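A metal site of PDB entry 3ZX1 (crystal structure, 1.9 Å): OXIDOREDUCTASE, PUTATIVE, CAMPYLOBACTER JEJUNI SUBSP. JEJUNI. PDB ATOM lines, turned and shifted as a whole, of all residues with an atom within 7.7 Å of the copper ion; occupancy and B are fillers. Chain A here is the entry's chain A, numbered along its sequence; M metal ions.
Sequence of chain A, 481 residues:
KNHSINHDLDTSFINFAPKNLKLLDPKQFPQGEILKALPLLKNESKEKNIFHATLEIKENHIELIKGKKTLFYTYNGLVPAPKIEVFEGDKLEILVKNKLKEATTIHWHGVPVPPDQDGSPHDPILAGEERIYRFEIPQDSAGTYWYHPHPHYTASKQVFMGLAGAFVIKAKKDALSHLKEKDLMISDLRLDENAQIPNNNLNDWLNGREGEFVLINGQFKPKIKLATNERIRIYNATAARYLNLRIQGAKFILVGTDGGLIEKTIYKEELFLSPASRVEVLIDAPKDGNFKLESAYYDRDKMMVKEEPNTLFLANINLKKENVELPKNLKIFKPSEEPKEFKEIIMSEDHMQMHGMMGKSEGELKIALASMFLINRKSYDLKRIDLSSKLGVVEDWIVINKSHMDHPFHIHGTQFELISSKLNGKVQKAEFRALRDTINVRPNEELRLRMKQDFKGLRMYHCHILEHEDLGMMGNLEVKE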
ATOM      1  N   LEU A 206      13.980 -22.084  25.036  1.00  0.00           N
ATOM      2  CA  LEU A 206      13.972 -21.755  26.472  1.00  0.00           C
ATOM      3  C   LEU A 206      13.372 -20.345  26.765  1.00  0.00           C
ATOM      4  O   LEU A 206      12.611 -20.162  27.729  1.00  0.00           O
ATOM      5  CB  LEU A 206      15.379 -21.820  27.030  1.00  0.00           C
ATOM      6  CG  LEU A 206      15.929 -23.248  27.237  1.00  0.00           C
ATOM      7  CD1 LEU A 206      17.443 -23.225  27.537  1.00  0.00           C
ATOM      8  CD2 LEU A 206      15.145 -23.975  28.303  1.00  0.00           C
ATOM      9  N   ASN A 207      13.741 -19.384  25.926  1.00  0.00           N
ATOM     10  CA  ASN A 207      13.479 -17.984  26.190  1.00  0.00           C
ATOM     11  C   ASN A 207      12.384 -17.344  25.342  1.00  0.00           C
ATOM     12  O   ASN A 207      11.897 -16.270  25.688  1.00  0.00           O
ATOM     13  CB  ASN A 207      14.772 -17.167  26.066  1.00  0.00           C
ATOM     14  CG  ASN A 207      15.814 -17.594  27.044  1.00  0.00           C
ATOM     15  OD1 ASN A 207      15.521 -17.926  28.216  1.00  0.00           O
ATOM     16  ND2 ASN A 207      17.062 -17.594  26.596  1.00  0.00           N
ATOM     17  N   GLY A 208      11.977 -18.008  24.268  1.00  0.00           N
ATOM     18  CA  GLY A 208      11.198 -17.347  23.217  1.00  0.00           C
ATOM     19  C   GLY A 208      12.241 -16.795  22.256  1.00  0.00           C
ATOM     20  O   GLY A 208      13.283 -16.264  22.673  1.00  0.00           O
ATOM     21  N   TYR A 242      10.466  -8.095  24.500  1.00  0.00           N
ATOM     22  CA  TYR A 242       9.893  -7.115  25.384  1.00  0.00           C
ATOM     23  C   TYR A 242      10.383  -5.727  24.962  1.00  0.00           C
ATOM     24  O   TYR A 242      11.592  -5.503  24.802  1.00  0.00           O
ATOM     25  CB  TYR A 242      10.331  -7.431  26.829  1.00  0.00           C
ATOM     26  CG  TYR A 242       9.508  -8.495  27.461  1.00  0.00           C
ATOM     27  CD1 TYR A 242       9.427  -9.780  26.897  1.00  0.00           C
ATOM     28  CD2 TYR A 242       8.770  -8.216  28.601  1.00  0.00           C
ATOM     29  CE1 TYR A 242       8.672 -10.774  27.476  1.00  0.00           C
ATOM     30  CE2 TYR A 242       8.006  -9.203  29.199  1.00  0.00           C
ATOM     31  CZ  TYR A 242       7.962 -10.469  28.633  1.00  0.00           C
ATOM     32  OH  TYR A 242       7.161 -11.397  29.199  1.00  0.00           O
ATOM     33  N   ARG A 300      14.464  -9.747  31.644  1.00  0.00           N
ATOM     34  CA  ARG A 300      13.372 -10.681  31.879  1.00  0.00           C
ATOM     35  C   ARG A 300      13.839 -12.070  32.298  1.00  0.00           C
ATOM     36  O   ARG A 300      13.066 -13.040  32.253  1.00  0.00           O
ATOM     37  CB  ARG A 300      12.428 -10.751  30.662  1.00  0.00           C
ATOM     38  CG  ARG A 300      13.016 -11.297  29.348  1.00  0.00           C
ATOM     39  CD  ARG A 300      11.884 -11.262  28.288  1.00  0.00           C
ATOM     40  NE  ARG A 300      12.254 -11.791  26.965  1.00  0.00           N
ATOM     41  CZ  ARG A 300      12.280 -13.081  26.656  1.00  0.00           C
ATOM     42  NH1 ARG A 300      11.977 -14.017  27.550  1.00  0.00           N
ATOM     43  NH2 ARG A 300      12.630 -13.437  25.415  1.00  0.00           N
ATOM     44  N   MET A 347       1.538 -19.909  36.844  1.00  0.00           N
ATOM     45  CA  MET A 347       2.477 -20.214  35.801  1.00  0.00           C
ATOM     46  C   MET A 347       3.793 -20.645  36.464  1.00  0.00           C
ATOM     47  O   MET A 347       4.266 -19.994  37.385  1.00  0.00           O
ATOM     48  CB  MET A 347       2.677 -19.004  34.901  1.00  0.00           C
ATOM     49  CG  MET A 347       1.362 -18.433  34.353  1.00  0.00           C
ATOM     50  SD  MET A 347       1.656 -16.923  33.393  1.00  0.00           S
ATOM     51  CE  MET A 347       1.830 -17.700  31.807  1.00  0.00           C
ATOM     52  N   SER A 348       4.376 -21.737  36.001  1.00  0.00           N
ATOM     53  CA  SER A 348       5.579 -22.265  36.675  1.00  0.00           C
ATOM     54  C   SER A 348       6.484 -22.963  35.653  1.00  0.00           C
ATOM     55  O   SER A 348       6.095 -23.128  34.482  1.00  0.00           O
ATOM     56  CB  SER A 348       5.217 -23.158  37.868  1.00  0.00           C
ATOM     57  OG  SER A 348       4.631 -24.408  37.487  1.00  0.00           O
ATOM     58  N   GLU A 349       7.691 -23.310  36.087  1.00  0.00           N
ATOM     59  CA  GLU A 349       8.612 -24.099  35.265  1.00  0.00           C
ATOM     60  C   GLU A 349       9.199 -25.244  36.086  1.00  0.00           C
ATOM     61  O   GLU A 349       9.346 -25.142  37.297  1.00  0.00           O
ATOM     62  CB  GLU A 349       9.751 -23.247  34.727  1.00  0.00           C
ATOM     63  CG  GLU A 349       9.281 -22.200  33.736  1.00  0.00           C
ATOM     64  CD  GLU A 349      10.294 -21.081  33.554  1.00  0.00           C
ATOM     65  OE1 GLU A 349      11.513 -21.350  33.558  1.00  0.00           O
ATOM     66  OE2 GLU A 349       9.867 -19.938  33.386  1.00  0.00           O
ATOM     67  N   PHE A 373       7.348 -26.076  30.914  1.00  0.00           N
ATOM     68  CA  PHE A 373       6.588 -24.824  31.071  1.00  0.00           C
ATOM     69  C   PHE A 373       5.144 -25.197  31.388  1.00  0.00           C
ATOM     70  O   PHE A 373       4.446 -25.764  30.533  1.00  0.00           O
ATOM     71  CB  PHE A 373       6.713 -24.028  29.773  1.00  0.00           C
ATOM     72  CG  PHE A 373       8.100 -23.515  29.518  1.00  0.00           C
ATOM     73  CD1 PHE A 373       8.583 -22.396  30.196  1.00  0.00           C
ATOM     74  CD2 PHE A 373       8.937 -24.134  28.603  1.00  0.00           C
ATOM     75  CE1 PHE A 373       9.880 -21.908  29.983  1.00  0.00           C
ATOM     76  CE2 PHE A 373      10.224 -23.664  28.377  1.00  0.00           C
ATOM     77  CZ  PHE A 373      10.712 -22.564  29.074  1.00  0.00           C
ATOM     78  N   ASN A 401       2.780 -15.767  38.761  1.00  0.00           N
ATOM     79  CA  ASN A 401       3.968 -16.280  38.136  1.00  0.00           C
ATOM     80  C   ASN A 401       4.960 -16.814  39.177  1.00  0.00           C
ATOM     81  O   ASN A 401       5.672 -16.049  39.806  1.00  0.00           O
ATOM     82  CB  ASN A 401       4.597 -15.189  37.276  1.00  0.00           C
ATOM     83  CG  ASN A 401       5.764 -15.673  36.475  1.00  0.00           C
ATOM     84  OD1 ASN A 401       6.157 -16.824  36.554  1.00  0.00           O
ATOM     85  ND2 ASN A 401       6.350 -14.774  35.703  1.00  0.00           N
ATOM     86  N   SER A 403       7.580 -18.655  38.496  1.00  0.00           N
ATOM     87  CA  SER A 403       8.843 -18.991  37.879  1.00  0.00           C
ATOM     88  C   SER A 403       9.777 -17.807  37.974  1.00  0.00           C
ATOM     89  O   SER A 403       9.364 -16.704  38.337  1.00  0.00           O
ATOM     90  CB  SER A 403       8.626 -19.341  36.409  1.00  0.00           C
ATOM     91  OG  SER A 403       8.434 -18.149  35.678  1.00  0.00           O
ATOM     92  N   MET A 405      11.162 -16.161  35.537  1.00  0.00           N
ATOM     93  CA  MET A 405      11.204 -15.317  34.330  1.00  0.00           C
ATOM     94  C   MET A 405       9.830 -14.775  33.952  1.00  0.00           C
ATOM     95  O   MET A 405       8.833 -15.381  34.304  1.00  0.00           O
ATOM     96  CB  MET A 405      11.838 -16.087  33.149  1.00  0.00           C
ATOM     97  CG  MET A 405      10.872 -17.037  32.445  1.00  0.00           C
ATOM     98  SD  MET A 405      11.609 -18.139  31.204  1.00  0.00           S
ATOM     99  CE  MET A 405      12.260 -16.950  30.020  1.00  0.00           C
ATOM    100  N   ASP A 406       9.765 -13.603  33.325  1.00  0.00           N
ATOM    101  CA  ASP A 406       8.479 -13.002  32.928  1.00  0.00           C
ATOM    102  C   ASP A 406       7.734 -13.939  31.951  1.00  0.00           C
ATOM    103  O   ASP A 406       8.380 -14.661  31.144  1.00  0.00           O
ATOM    104  CB  ASP A 406       8.669 -11.645  32.273  1.00  0.00           C
ATOM    105  CG  ASP A 406       9.397 -10.639  33.161  1.00  0.00           C
ATOM    106  OD1 ASP A 406      10.529 -10.935  33.646  1.00  0.00           O
ATOM    107  OD2 ASP A 406       8.833  -9.542  33.341  1.00  0.00           O
ATOM    108  N   HIS A 407       6.407 -13.978  32.033  1.00  0.00           N
ATOM    109  CA  HIS A 407       5.592 -14.613  30.997  1.00  0.00           C
ATOM    110  C   HIS A 407       4.385 -13.738  30.761  1.00  0.00           C
ATOM    111  O   HIS A 407       3.677 -13.366  31.751  1.00  0.00           O
ATOM    112  CB  HIS A 407       5.082 -15.990  31.375  1.00  0.00           C
ATOM    113  CG  HIS A 407       6.145 -16.940  31.802  1.00  0.00           C
ATOM    114  ND1 HIS A 407       6.821 -17.739  30.902  1.00  0.00           N
ATOM    115  CD2 HIS A 407       6.625 -17.260  33.030  1.00  0.00           C
ATOM    116  CE1 HIS A 407       7.692 -18.481  31.556  1.00  0.00           C
ATOM    117  NE2 HIS A 407       7.589 -18.218  32.856  1.00  0.00           N
ATOM    118  N   PRO A 408       4.110 -13.433  29.488  1.00  0.00           N
ATOM    119  CA  PRO A 408       2.914 -12.609  29.230  1.00  0.00           C
ATOM    120  C   PRO A 408       1.671 -13.507  29.081  1.00  0.00           C
ATOM    121  O   PRO A 408       1.660 -14.395  28.237  1.00  0.00           O
ATOM    122  CB  PRO A 408       3.259 -11.852  27.930  1.00  0.00           C
ATOM    123  CG  PRO A 408       4.228 -12.808  27.143  1.00  0.00           C
ATOM    124  CD  PRO A 408       4.893 -13.712  28.255  1.00  0.00           C
ATOM    125  N   PHE A 409       0.653 -13.284  29.908  1.00  0.00           N
ATOM    126  CA  PHE A 409      -0.534 -14.125  29.937  1.00  0.00           C
ATOM    127  C   PHE A 409      -1.581 -13.655  28.931  1.00  0.00           C
ATOM    128  O   PHE A 409      -1.885 -12.467  28.883  1.00  0.00           O
ATOM    129  CB  PHE A 409      -1.174 -14.050  31.334  1.00  0.00           C
ATOM    130  CG  PHE A 409      -2.542 -14.693  31.418  1.00  0.00           C
ATOM    131  CD1 PHE A 409      -2.664 -16.090  31.582  1.00  0.00           C
ATOM    132  CD2 PHE A 409      -3.713 -13.920  31.364  1.00  0.00           C
ATOM    133  CE1 PHE A 409      -3.935 -16.713  31.707  1.00  0.00           C
ATOM    134  CE2 PHE A 409      -4.984 -14.522  31.439  1.00  0.00           C
ATOM    135  CZ  PHE A 409      -5.100 -15.938  31.623  1.00  0.00           C
ATOM    136  N   HIS A 462      -2.931 -18.903  27.778  1.00  0.00           N
ATOM    137  CA  HIS A 462      -1.559 -19.421  27.667  1.00  0.00           C
ATOM    138  C   HIS A 462      -0.586 -18.317  27.834  1.00  0.00           C
ATOM    139  O   HIS A 462      -0.958 -17.141  27.853  1.00  0.00           O
ATOM    140  CB  HIS A 462      -1.325 -20.104  26.295  1.00  0.00           C
ATOM    141  CG  HIS A 462      -1.794 -19.277  25.122  1.00  0.00           C
ATOM    142  ND1 HIS A 462      -0.930 -18.523  24.350  1.00  0.00           N
ATOM    143  CD2 HIS A 462      -3.024 -19.103  24.597  1.00  0.00           C
ATOM    144  CE1 HIS A 462      -1.623 -17.928  23.380  1.00  0.00           C
ATOM    145  NE2 HIS A 462      -2.887 -18.251  23.511  1.00  0.00           N
ATOM    146  N   CYS A 463       0.666 -18.701  28.018  1.00  0.00           N
ATOM    147  CA  CYS A 463       1.763 -17.763  27.898  1.00  0.00           C
ATOM    148  C   CYS A 463       1.841 -17.360  26.435  1.00  0.00           C
ATOM    149  O   CYS A 463       1.623 -18.201  25.566  1.00  0.00           O
ATOM    150  CB  CYS A 463       3.086 -18.424  28.276  1.00  0.00           C
ATOM    151  SG  CYS A 463       4.410 -17.308  27.969  1.00  0.00           S
ATOM    152  N   HIS A 464       2.110 -16.101  26.165  1.00  0.00           N
ATOM    153  CA  HIS A 464       2.162 -15.665  24.782  1.00  0.00           C
ATOM    154  C   HIS A 464       3.615 -15.507  24.284  1.00  0.00           C
ATOM    155  O   HIS A 464       3.835 -14.917  23.212  1.00  0.00           O
ATOM    156  CB  HIS A 464       1.296 -14.411  24.490  1.00  0.00           C
ATOM    157  CG  HIS A 464       0.721 -14.420  23.103  1.00  0.00           C
ATOM    158  ND1 HIS A 464       1.500 -14.231  21.980  1.00  0.00           N
ATOM    159  CD2 HIS A 464      -0.528 -14.688  22.649  1.00  0.00           C
ATOM    160  CE1 HIS A 464       0.759 -14.348  20.900  1.00  0.00           C
ATOM    161  NE2 HIS A 464      -0.476 -14.617  21.276  1.00  0.00           N
ATOM    162  N   ILE A 465       4.584 -16.024  25.037  1.00  0.00           N
ATOM    163  CA  ILE A 465       5.892 -16.279  24.436  1.00  0.00           C
ATOM    164  C   ILE A 465       5.654 -17.541  23.599  1.00  0.00           C
ATOM    165  O   ILE A 465       5.395 -18.618  24.142  1.00  0.00           O
ATOM    166  CB  ILE A 465       7.030 -16.447  25.485  1.00  0.00           C
ATOM    167  CG1 ILE A 465       7.426 -15.069  26.076  1.00  0.00           C
ATOM    168  CG2 ILE A 465       8.257 -17.145  24.831  1.00  0.00           C
ATOM    169  CD1 ILE A 465       8.121 -15.143  27.448  1.00  0.00           C
ATOM    170  N   LEU A 466       5.684 -17.389  22.280  1.00  0.00           N
ATOM    171  CA  LEU A 466       5.143 -18.418  21.395  1.00  0.00           C
ATOM    172  C   LEU A 466       5.828 -19.750  21.595  1.00  0.00           C
ATOM    173  O   LEU A 466       5.166 -20.784  21.575  1.00  0.00           O
ATOM    174  CB  LEU A 466       5.237 -17.995  19.916  1.00  0.00           C
ATOM    175  CG  LEU A 466       4.383 -16.782  19.521  1.00  0.00           C
ATOM    176  CD1 LEU A 466       4.468 -16.592  18.031  1.00  0.00           C
ATOM    177  CD2 LEU A 466       2.924 -16.911  19.877  1.00  0.00           C
ATOM    178  N   GLU A 467       7.134 -19.750  21.843  1.00  0.00           N
ATOM    179  CA  GLU A 467       7.811 -21.018  22.026  1.00  0.00           C
ATOM    180  C   GLU A 467       7.303 -21.739  23.288  1.00  0.00           C
ATOM    181  O   GLU A 467       7.178 -22.970  23.282  1.00  0.00           O
ATOM    182  CB  GLU A 467       9.329 -20.872  22.071  1.00  0.00           C
ATOM    183  CG  GLU A 467      10.029 -20.617  20.735  1.00  0.00           C
ATOM    184  CD  GLU A 467       9.678 -19.294  20.076  1.00  0.00           C
ATOM    185  OE1 GLU A 467       9.229 -18.330  20.768  1.00  0.00           O
ATOM    186  OE2 GLU A 467       9.833 -19.232  18.834  1.00  0.00           O
ATOM    187  N   HIS A 468       6.984 -20.982  24.354  1.00  0.00           N
ATOM    188  CA  HIS A 468       6.431 -21.592  25.597  1.00  0.00           C
ATOM    189  C   HIS A 468       5.049 -22.180  25.366  1.00  0.00           C
ATOM    190  O   HIS A 468       4.746 -23.305  25.815  1.00  0.00           O
ATOM    191  CB  HIS A 468       6.340 -20.561  26.740  1.00  0.00           C
ATOM    192  CG  HIS A 468       7.675 -20.063  27.179  1.00  0.00           C
ATOM    193  ND1 HIS A 468       7.824 -19.098  28.147  1.00  0.00           N
ATOM    194  CD2 HIS A 468       8.937 -20.407  26.786  1.00  0.00           C
ATOM    195  CE1 HIS A 468       9.116 -18.857  28.331  1.00  0.00           C
ATOM    196  NE2 HIS A 468       9.810 -19.644  27.528  1.00  0.00           N
ATOM    197  N   GLU A 469       4.229 -21.433  24.631  1.00  0.00           N
ATOM    198  CA  GLU A 469       2.915 -21.918  24.218  1.00  0.00           C
ATOM    199  C   GLU A 469       3.042 -23.253  23.485  1.00  0.00           C
ATOM    200  O   GLU A 469       2.370 -24.205  23.858  1.00  0.00           O
ATOM    201  CB  GLU A 469       2.185 -20.851  23.394  1.00  0.00           C
ATOM    202  CG  GLU A 469       1.197 -21.318  22.350  1.00  0.00           C
ATOM    203  CD  GLU A 469       0.881 -20.187  21.354  1.00  0.00           C
ATOM    204  OE1 GLU A 469       0.781 -19.026  21.782  1.00  0.00           O
ATOM    205  OE2 GLU A 469       0.766 -20.454  20.145  1.00  0.00           O
ATOM    206  N   MET A 473       2.597 -24.529  27.448  1.00  0.00           N
ATOM    207  CA  MET A 473       2.267 -23.618  28.546  1.00  0.00           C
ATOM    208  C   MET A 473       0.924 -22.988  28.274  1.00  0.00           C
ATOM    209  O   MET A 473       0.833 -21.790  27.991  1.00  0.00           O
ATOM    210  CB  MET A 473       3.352 -22.555  28.730  1.00  0.00           C
ATOM    211  CG  MET A 473       3.261 -21.816  30.104  1.00  0.00           C
ATOM    212  SD  MET A 473       4.698 -20.752  30.426  1.00  0.00           S
ATOM    213  CE  MET A 473       4.530 -20.549  32.189  1.00  0.00           C
HETATM  214 CU    CU M   1       6.283 -18.146  28.998  1.00  0.00          CU
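O of Met 473 is in hydrogen-bond range of N of Cys 463, 3.1 Å away. ND1 of His 407 sits close to SD of Met 473 (3.7 Å). A ring nitrogen (NE2) of His 407 sits at hydrogen-bond distance from the side-chain hydroxyl of Ser 403. O of Met 405 sits close to NE2 of His 407. NE2 of His 407 lies within hydrogen-bond range of OE2 of Glu 349 (2.9 Å). A ring nitrogen (NE2) of His 468 is in hydrogen-bond range of the backbone carbonyl oxygen (O) of Leu 206, 2.9 Å away. O of His 468 is in hydrogen-bond range of N of Met 473 (3.0 Å). SG of Cys 463 sits close to N of Ile 465 (3.2 Å).
The copper ion is bound by ND1 of His 468 (2.0 Å). A ring nitrogen (ND1) of His 407 binds the copper ion (2.0 Å). SG of Cys 463 binds the copper ion, at 2.3 Å.
Ile 465 touches the copper ion (CD1 to CU, 3.8 Å). SD of Met 473 touches the copper ion, at 3.4 Å.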
